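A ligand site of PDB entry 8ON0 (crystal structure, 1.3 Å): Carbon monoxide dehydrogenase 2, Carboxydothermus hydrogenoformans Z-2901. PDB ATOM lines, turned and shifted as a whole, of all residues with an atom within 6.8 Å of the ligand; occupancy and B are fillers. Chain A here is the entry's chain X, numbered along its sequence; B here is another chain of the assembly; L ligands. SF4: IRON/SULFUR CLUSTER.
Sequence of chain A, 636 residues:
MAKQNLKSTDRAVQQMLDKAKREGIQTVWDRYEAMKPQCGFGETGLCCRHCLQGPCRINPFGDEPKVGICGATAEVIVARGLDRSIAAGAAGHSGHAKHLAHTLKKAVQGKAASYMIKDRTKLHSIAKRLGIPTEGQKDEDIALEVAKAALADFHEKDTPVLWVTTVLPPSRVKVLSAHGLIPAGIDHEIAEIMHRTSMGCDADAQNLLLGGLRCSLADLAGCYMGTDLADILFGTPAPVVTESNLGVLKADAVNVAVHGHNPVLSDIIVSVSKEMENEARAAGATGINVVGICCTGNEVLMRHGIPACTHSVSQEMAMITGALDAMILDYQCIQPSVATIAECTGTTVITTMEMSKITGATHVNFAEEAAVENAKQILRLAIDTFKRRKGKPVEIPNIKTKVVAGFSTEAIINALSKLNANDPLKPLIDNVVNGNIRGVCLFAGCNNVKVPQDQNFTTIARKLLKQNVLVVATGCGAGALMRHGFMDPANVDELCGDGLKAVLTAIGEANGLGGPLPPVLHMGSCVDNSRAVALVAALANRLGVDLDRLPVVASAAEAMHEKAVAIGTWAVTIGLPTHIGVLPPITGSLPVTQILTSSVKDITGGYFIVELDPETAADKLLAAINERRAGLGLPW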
ATOM      1  N   CYS A  47     -28.493   3.973 -20.939  1.00  0.00           N
ATOM      2  CA  CYS A  47     -27.774   3.616 -19.717  1.00  0.00           C
ATOM      3  C   CYS A  47     -28.741   2.847 -18.841  1.00  0.00           C
ATOM      4  O   CYS A  47     -29.928   3.194 -18.739  1.00  0.00           O
ATOM      5  CB  CYS A  47     -27.273   4.834 -18.980  1.00  0.00           C
ATOM      6  SG  CYS A  47     -26.372   4.364 -17.468  1.00  0.00           S
ATOM      7  N   CYS A  48     -28.222   1.775 -18.228  1.00  0.00           N
ATOM      8  CA  CYS A  48     -28.981   0.957 -17.293  1.00  0.00           C
ATOM      9  C   CYS A  48     -28.142   0.662 -16.070  1.00  0.00           C
ATOM     10  O   CYS A  48     -26.983   0.266 -16.189  1.00  0.00           O
ATOM     11  CB  CYS A  48     -29.385  -0.364 -17.949  1.00  0.00           C
ATOM     12  SG  CYS A  48     -30.353  -1.436 -16.893  1.00  0.00           S
ATOM     13  N   ARG A  49     -28.742   0.831 -14.896  1.00  0.00           N
ATOM     14  CA  ARG A  49     -28.158   0.506 -13.597  1.00  0.00           C
ATOM     15  C   ARG A  49     -29.099  -0.400 -12.801  1.00  0.00           C
ATOM     16  O   ARG A  49     -29.132  -0.341 -11.562  1.00  0.00           O
ATOM     17  CB  ARG A  49     -27.806   1.766 -12.807  1.00  0.00           C
ATOM     18  CG  ARG A  49     -26.744   2.622 -13.488  1.00  0.00           C
ATOM     19  CD  ARG A  49     -26.627   3.986 -12.843  1.00  0.00           C
ATOM     20  NE  ARG A  49     -26.321   3.835 -11.435  1.00  0.00           N
ATOM     21  CZ  ARG A  49     -26.576   4.722 -10.487  1.00  0.00           C
ATOM     22  NH1 ARG A  49     -27.164   5.881 -10.746  1.00  0.00           N
ATOM     23  NH2 ARG A  49     -26.225   4.439  -9.234  1.00  0.00           N
ATOM     24  N   HIS A  50     -29.886  -1.223 -13.489  1.00  0.00           N
ATOM     25  CA  HIS A  50     -30.884  -2.054 -12.826  1.00  0.00           C
ATOM     26  C   HIS A  50     -30.305  -3.297 -12.179  1.00  0.00           C
ATOM     27  O   HIS A  50     -31.050  -4.045 -11.540  1.00  0.00           O
ATOM     28  CB  HIS A  50     -32.034  -2.400 -13.773  1.00  0.00           C
ATOM     29  CG  HIS A  50     -32.877  -1.218 -14.175  1.00  0.00           C
ATOM     30  ND1 HIS A  50     -34.135  -1.364 -14.729  1.00  0.00           N
ATOM     31  CD2 HIS A  50     -32.626   0.122 -14.179  1.00  0.00           C
ATOM     32  CE1 HIS A  50     -34.624  -0.180 -15.027  1.00  0.00           C
ATOM     33  NE2 HIS A  50     -33.743   0.746 -14.686  1.00  0.00           N
ATOM     34  N   CYS A  51     -29.006  -3.523 -12.285  1.00  0.00           N
ATOM     35  CA  CYS A  51     -28.365  -4.570 -11.484  1.00  0.00           C
ATOM     36  C   CYS A  51     -26.901  -4.244 -11.263  1.00  0.00           C
ATOM     37  O   CYS A  51     -26.347  -3.331 -11.854  1.00  0.00           O
ATOM     38  CB  CYS A  51     -28.544  -5.979 -12.071  1.00  0.00           C
ATOM     39  SG  CYS A  51     -27.387  -6.428 -13.378  1.00  0.00           S
ATOM     40  N   LEU A  52     -26.303  -4.971 -10.325  1.00  0.00           N
ATOM     41  CA  LEU A  52     -24.933  -4.719  -9.923  1.00  0.00           C
ATOM     42  C   LEU A  52     -23.896  -5.253 -10.897  1.00  0.00           C
ATOM     43  O   LEU A  52     -22.690  -5.145 -10.609  1.00  0.00           O
ATOM     44  CB  LEU A  52     -24.686  -5.320  -8.519  1.00  0.00           C
ATOM     45  CG  LEU A  52     -25.585  -4.771  -7.423  1.00  0.00           C
ATOM     46  CD1 LEU A  52     -25.262  -5.398  -6.093  1.00  0.00           C
ATOM     47  CD2 LEU A  52     -25.472  -3.251  -7.357  1.00  0.00           C
ATOM     48  N   GLN A  53     -24.303  -5.818 -12.032  1.00  0.00           N
ATOM     49  CA  GLN A  53     -23.373  -6.027 -13.132  1.00  0.00           C
ATOM     50  C   GLN A  53     -23.108  -4.747 -13.928  1.00  0.00           C
ATOM     51  O   GLN A  53     -22.104  -4.676 -14.639  1.00  0.00           O
ATOM     52  CB  GLN A  53     -23.889  -7.103 -14.087  1.00  0.00           C
ATOM     53  CG  GLN A  53     -23.966  -8.442 -13.415  1.00  0.00           C
ATOM     54  CD  GLN A  53     -24.429  -9.573 -14.277  1.00  0.00           C
ATOM     55  OE1 GLN A  53     -23.951 -10.688 -14.119  1.00  0.00           O
ATOM     56  NE2 GLN A  53     -25.360  -9.322 -15.180  1.00  0.00           N
ATOM     57  N   GLY A  54     -24.000  -3.761 -13.812  1.00  0.00           N
ATOM     58  CA  GLY A  54     -23.832  -2.502 -14.491  1.00  0.00           C
ATOM     59  C   GLY A  54     -22.835  -1.610 -13.781  1.00  0.00           C
ATOM     60  O   GLY A  54     -22.159  -2.003 -12.828  1.00  0.00           O
ATOM     61  N   PRO A  55     -22.760  -0.366 -14.240  1.00  0.00           N
ATOM     62  CA  PRO A  55     -23.652   0.254 -15.202  1.00  0.00           C
ATOM     63  C   PRO A  55     -23.364  -0.265 -16.590  1.00  0.00           C
ATOM     64  O   PRO A  55     -22.230  -0.537 -16.981  1.00  0.00           O
ATOM     65  CB  PRO A  55     -23.276   1.730 -15.173  1.00  0.00           C
ATOM     66  CG  PRO A  55     -22.298   1.910 -14.140  1.00  0.00           C
ATOM     67  CD  PRO A  55     -21.913   0.604 -13.548  1.00  0.00           C
ATOM     68  N   CYS A  56     -24.422  -0.426 -17.357  1.00  0.00           N
ATOM     69  CA  CYS A  56     -24.349  -0.743 -18.768  1.00  0.00           C
ATOM     70  C   CYS A  56     -24.722   0.488 -19.568  1.00  0.00           C
ATOM     71  O   CYS A  56     -25.626   1.229 -19.212  1.00  0.00           O
ATOM     72  CB  CYS A  56     -25.307  -1.873 -19.089  1.00  0.00           C
ATOM     73  SG  CYS A  56     -24.748  -3.472 -18.427  1.00  0.00           S
ATOM     74  N   ARG A  57     -23.984   0.729 -20.628  1.00  0.00           N
ATOM     75  CA  ARG A  57     -24.321   1.773 -21.564  1.00  0.00           C
ATOM     76  C   ARG A  57     -24.261   1.181 -22.966  1.00  0.00           C
ATOM     77  O   ARG A  57     -23.684   0.105 -23.186  1.00  0.00           O
ATOM     78  CB  ARG A  57     -23.339   2.915 -21.420  1.00  0.00           C
ATOM     79  CG  ARG A  57     -22.003   2.609 -22.009  1.00  0.00           C
ATOM     80  CD  ARG A  57     -20.894   3.486 -21.455  1.00  0.00           C
ATOM     81  NE  ARG A  57     -19.623   3.086 -22.045  1.00  0.00           N
ATOM     82  CZ  ARG A  57     -18.909   2.037 -21.678  1.00  0.00           C
ATOM     83  NH1 ARG A  57     -19.308   1.226 -20.692  1.00  0.00           N
ATOM     84  NH2 ARG A  57     -17.776   1.760 -22.326  1.00  0.00           N
ATOM     85  N   VAL A  67     -25.038  -3.689 -26.595  1.00  0.00           N
ATOM     86  CA  VAL A  67     -26.072  -4.435 -25.882  1.00  0.00           C
ATOM     87  C   VAL A  67     -25.665  -4.486 -24.417  1.00  0.00           C
ATOM     88  O   VAL A  67     -24.479  -4.441 -24.094  1.00  0.00           O
ATOM     89  CB  VAL A  67     -26.203  -5.842 -26.512  1.00  0.00           C
ATOM     90  CG1 VAL A  67     -24.888  -6.633 -26.429  1.00  0.00           C
ATOM     91  CG2 VAL A  67     -27.309  -6.640 -25.905  1.00  0.00           C
ATOM     92  N   GLY A  68     -26.650  -4.580 -23.524  1.00  0.00           N
ATOM     93  CA  GLY A  68     -26.340  -4.691 -22.127  1.00  0.00           C
ATOM     94  C   GLY A  68     -25.732  -6.053 -21.796  1.00  0.00           C
ATOM     95  O   GLY A  68     -25.850  -7.011 -22.559  1.00  0.00           O
ATOM     96  N   ILE A  69     -25.117  -6.140 -20.612  1.00  0.00           N
ATOM     97  CA  ILE A  69     -24.393  -7.359 -20.239  1.00  0.00           C
ATOM     98  C   ILE A  69     -25.337  -8.556 -20.204  1.00  0.00           C
ATOM     99  O   ILE A  69     -24.959  -9.654 -20.625  1.00  0.00           O
ATOM    100  CB  ILE A  69     -23.657  -7.154 -18.908  1.00  0.00           C
ATOM    101  CG1 ILE A  69     -22.434  -6.235 -19.139  1.00  0.00           C
ATOM    102  CG2 ILE A  69     -23.255  -8.496 -18.306  1.00  0.00           C
ATOM    103  CD1 ILE A  69     -21.826  -5.690 -17.874  1.00  0.00           C
ATOM    104  N   CYS A  70     -26.572  -8.369 -19.722  1.00  0.00           N
ATOM    105  CA  CYS A  70     -27.531  -9.461 -19.628  1.00  0.00           C
ATOM    106  C   CYS A  70     -28.192  -9.761 -20.962  1.00  0.00           C
ATOM    107  O   CYS A  70     -28.986 -10.707 -21.049  1.00  0.00           O
ATOM    108  CB  CYS A  70     -28.590  -9.093 -18.615  1.00  0.00           C
ATOM    109  SG  CYS A  70     -29.545  -7.618 -19.102  1.00  0.00           S
ATOM    110  N   GLY A  71     -27.906  -8.975 -22.001  1.00  0.00           N
ATOM    111  CA  GLY A  71     -28.566  -9.105 -23.295  1.00  0.00           C
ATOM    112  C   GLY A  71     -29.638  -8.076 -23.554  1.00  0.00           C
ATOM    113  O   GLY A  71     -30.273  -8.123 -24.609  1.00  0.00           O
ATOM    114  N   ALA A  72     -29.865  -7.148 -22.619  1.00  0.00           N
ATOM    115  CA  ALA A  72     -30.889  -6.127 -22.811  1.00  0.00           C
ATOM    116  C   ALA A  72     -30.518  -5.226 -23.979  1.00  0.00           C
ATOM    117  O   ALA A  72     -29.429  -4.663 -24.031  1.00  0.00           O
ATOM    118  CB  ALA A  72     -31.040  -5.298 -21.535  1.00  0.00           C
ATOM    119  N   ILE A  77     -33.747  -1.287 -22.754  1.00  0.00           N
ATOM    120  CA  ILE A  77     -33.185  -0.372 -21.762  1.00  0.00           C
ATOM    121  C   ILE A  77     -33.961   0.948 -21.785  1.00  0.00           C
ATOM    122  O   ILE A  77     -34.380   1.466 -20.747  1.00  0.00           O
ATOM    123  CB  ILE A  77     -31.678  -0.148 -22.026  1.00  0.00           C
ATOM    124  CG1 ILE A  77     -30.943  -1.435 -21.628  1.00  0.00           C
ATOM    125  CG2 ILE A  77     -31.158   1.092 -21.330  1.00  0.00           C
ATOM    126  CD1 ILE A  77     -29.448  -1.501 -22.005  1.00  0.00           C
ATOM    127  N   ARG A  80     -37.557   0.401 -20.374  1.00  0.00           N
ATOM    128  CA  ARG A  80     -37.553   0.166 -18.924  1.00  0.00           C
ATOM    129  C   ARG A  80     -37.305   1.472 -18.148  1.00  0.00           C
ATOM    130  O   ARG A  80     -37.979   1.746 -17.147  1.00  0.00           O
ATOM    131  CB  ARG A  80     -36.510  -0.896 -18.559  1.00  0.00           C
ATOM    132  CG  ARG A  80     -36.850  -2.280 -19.080  1.00  0.00           C
ATOM    133  CD  ARG A  80     -35.987  -3.340 -18.494  1.00  0.00           C
ATOM    134  NE  ARG A  80     -34.559  -3.070 -18.634  1.00  0.00           N
ATOM    135  CZ  ARG A  80     -33.630  -4.000 -18.389  1.00  0.00           C
ATOM    136  NH1 ARG A  80     -33.949  -5.245 -18.092  1.00  0.00           N
ATOM    137  NH2 ARG A  80     -32.341  -3.661 -18.483  1.00  0.00           N
ATOM    138  N   THR A 197     -39.619  -4.147 -14.876  1.00  0.00           N
ATOM    139  CA  THR A 197     -38.437  -3.453 -15.376  1.00  0.00           C
ATOM    140  C   THR A 197     -37.145  -3.874 -14.672  1.00  0.00           C
ATOM    141  O   THR A 197     -36.063  -3.406 -15.071  1.00  0.00           O
ATOM    142  CB  THR A 197     -38.601  -1.923 -15.253  1.00  0.00           C
ATOM    143  OG1 THR A 197     -38.841  -1.566 -13.894  1.00  0.00           O
ATOM    144  CG2 THR A 197     -39.752  -1.399 -16.167  1.00  0.00           C
ATOM    145  N   SER A 198     -37.233  -4.660 -13.609  1.00  0.00           N
ATOM    146  CA  SER A 198     -36.035  -5.170 -12.961  1.00  0.00           C
ATOM    147  C   SER A 198     -35.333  -6.187 -13.864  1.00  0.00           C
ATOM    148  O   SER A 198     -35.859  -6.619 -14.898  1.00  0.00           O
ATOM    149  CB  SER A 198     -36.383  -5.746 -11.568  1.00  0.00           C
ATOM    150  OG  SER A 198     -37.028  -7.019 -11.634  1.00  0.00           O
ATOM    151  N   MET A 199     -34.118  -6.568 -13.449  1.00  0.00           N
ATOM    152  CA  MET A 199     -33.295  -7.403 -14.320  1.00  0.00           C
ATOM    153  C   MET A 199     -33.967  -8.731 -14.612  1.00  0.00           C
ATOM    154  O   MET A 199     -34.493  -9.401 -13.722  1.00  0.00           O
ATOM    155  CB  MET A 199     -31.880  -7.528 -13.764  1.00  0.00           C
ATOM    156  CG  MET A 199     -30.911  -8.395 -14.553  1.00  0.00           C
ATOM    157  SD  MET A 199     -31.167 -10.156 -14.292  1.00  0.00           S
ATOM    158  CE  MET A 199     -30.175 -10.844 -15.590  1.00  0.00           C
ATOM    159  N   GLY A 200     -33.893  -9.137 -15.872  1.00  0.00           N
ATOM    160  CA  GLY A 200     -34.318 -10.455 -16.244  1.00  0.00           C
ATOM    161  C   GLY A 200     -35.807 -10.689 -16.227  1.00  0.00           C
ATOM    162  O   GLY A 200     -36.257 -11.841 -16.108  1.00  0.00           O
ATOM    163  N   MET B  35     -18.238  -4.109 -22.501  1.00  0.00           N
ATOM    164  CA  MET B  35     -18.666  -2.972 -21.671  1.00  0.00           C
ATOM    165  C   MET B  35     -17.559  -2.302 -20.930  1.00  0.00           C
ATOM    166  O   MET B  35     -17.754  -1.193 -20.417  1.00  0.00           O
ATOM    167  CB  MET B  35     -19.738  -3.463 -20.713  1.00  0.00           C
ATOM    168  CG  MET B  35     -20.688  -2.460 -20.104  1.00  0.00           C
ATOM    169  SD  MET B  35     -21.599  -1.506 -21.309  1.00  0.00           S
ATOM    170  CE  MET B  35     -22.831  -2.772 -21.796  1.00  0.00           C
ATOM    171  N   GLN B  38     -16.288   0.258 -17.373  1.00  0.00           N
ATOM    172  CA  GLN B  38     -17.622   0.704 -17.040  1.00  0.00           C
ATOM    173  C   GLN B  38     -17.582   2.078 -16.379  1.00  0.00           C
ATOM    174  O   GLN B  38     -16.560   2.535 -15.847  1.00  0.00           O
ATOM    175  CB  GLN B  38     -18.328  -0.289 -16.131  1.00  0.00           C
ATOM    176  CG  GLN B  38     -18.529  -1.629 -16.812  1.00  0.00           C
ATOM    177  CD  GLN B  38     -19.181  -2.633 -15.918  1.00  0.00           C
ATOM    178  OE1 GLN B  38     -18.508  -3.392 -15.197  1.00  0.00           O
ATOM    179  NE2 GLN B  38     -20.509  -2.694 -16.003  1.00  0.00           N
ATOM    180  N   PRO B 336     -32.125 -11.878 -21.197  1.00  0.00           N
ATOM    181  CA  PRO B 336     -32.915 -11.876 -22.436  1.00  0.00           C
ATOM    182  C   PRO B 336     -32.140 -12.337 -23.653  1.00  0.00           C
ATOM    183  O   PRO B 336     -32.750 -12.625 -24.694  1.00  0.00           O
ATOM    184  CB  PRO B 336     -33.414 -10.420 -22.538  1.00  0.00           C
ATOM    185  CG  PRO B 336     -32.444  -9.639 -21.721  1.00  0.00           C
ATOM    186  CD  PRO B 336     -32.053 -10.534 -20.584  1.00  0.00           C
ATOM    187  N   MET B 560     -26.158  -9.603  -7.469  1.00  0.00           N
ATOM    188  CA  MET B 560     -26.426  -8.963  -8.752  1.00  0.00           C
ATOM    189  C   MET B 560     -27.750  -8.194  -8.749  1.00  0.00           C
ATOM    190  O   MET B 560     -27.799  -7.012  -9.054  1.00  0.00           O
ATOM    191  CB  MET B 560     -26.447 -10.019  -9.866  1.00  0.00           C
ATOM    192  CG  MET B 560     -26.753  -9.532 -11.272  1.00  0.00           C
ATOM    193  SD  MET B 560     -28.494  -9.646 -11.726  1.00  0.00           S
ATOM    194  CE  MET B 560     -28.767 -11.410 -11.661  1.00  0.00           C
HETATM  195 FE1  SF4 L   1     -26.666  -4.204 -17.427  1.00  0.00          FE
HETATM  196 FE2  SF4 L   1     -27.930  -5.221 -15.243  1.00  0.00          FE
HETATM  197 FE3  SF4 L   1     -29.122  -3.337 -16.795  1.00  0.00          FE
HETATM  198 FE4  SF4 L   1     -28.824  -5.854 -17.796  1.00  0.00          FE
HETATM  199  S1  SF4 L   1     -30.081  -5.212 -16.014  1.00  0.00           S
HETATM  200  S2  SF4 L   1     -28.403  -3.948 -18.839  1.00  0.00           S
HETATM  201  S3  SF4 L   1     -26.787  -6.328 -16.872  1.00  0.00           S
HETATM  202  S4  SF4 L   1     -27.255  -3.131 -15.484  1.00  0.00           S
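Residues that only touch the ligand: Met 199, His 50, Ile 69 and Gly 68.
Hydrophobic or aromatic side chains within 4 Å of the ligand: Ile 69 and Met 199.
The nearest printed residue that does not touch the ligand is Ala 72 (4.01 Å).
The backbone NH of Ile 69 sits close to the side-chain sulfur of Cys 56 (3.5 Å).
ND1 of His 50 lies within hydrogen-bond range of O of Thr 197, at 2.8 Å.
The side-chain sulfur (SD) of Met 560 of chain B sits close to the side-chain sulfur (SG) of Cys 51.
SG of Cys 51 lies close to N of Gln 53, 3.4 Å away.
The side-chain sulfur (SG) of Cys 70 sits close to the backbone NH (N) of Ala 72.
The backbone carbonyl oxygen (O) of Gln 53 is in hydrogen-bond range of the side-chain amide nitrogen (NE2) of Gln 38 of chain B, at 2.9 Å.
SG of Cys 48 lies close to N of His 50.
N of Cys 48 is in hydrogen-bond range of O of Cys 56.
The guanidinium group (NH2) of Arg 80 sits close to a sulfur (S1) of the ligand (3.7 Å).
An iron atom (FE4) of the ligand is bound by the side-chain sulfur (SG) of Cys 70, 2.3 Å away.
The backbone NH (N) of Cys 51 lies close to a sulfur (S4) of the ligand, at 3.7 Å.
FE1 of the ligand is bound by SG of Cys 56, at 2.3 Å.
The side-chain amide nitrogen (NE2) of Gln 53 lies close to a sulfur (S3) of the ligand (3.7 Å).
SG of Cys 48 binds FE3 of the ligand (2.3 Å).
FE2 of the ligand is bound by SG of Cys 51, 2.3 Å away.
S3 of the ligand lies close to N of Cys 70 (3.5 Å).
S4 of the ligand sits close to N of Gly 54 (3.7 Å).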
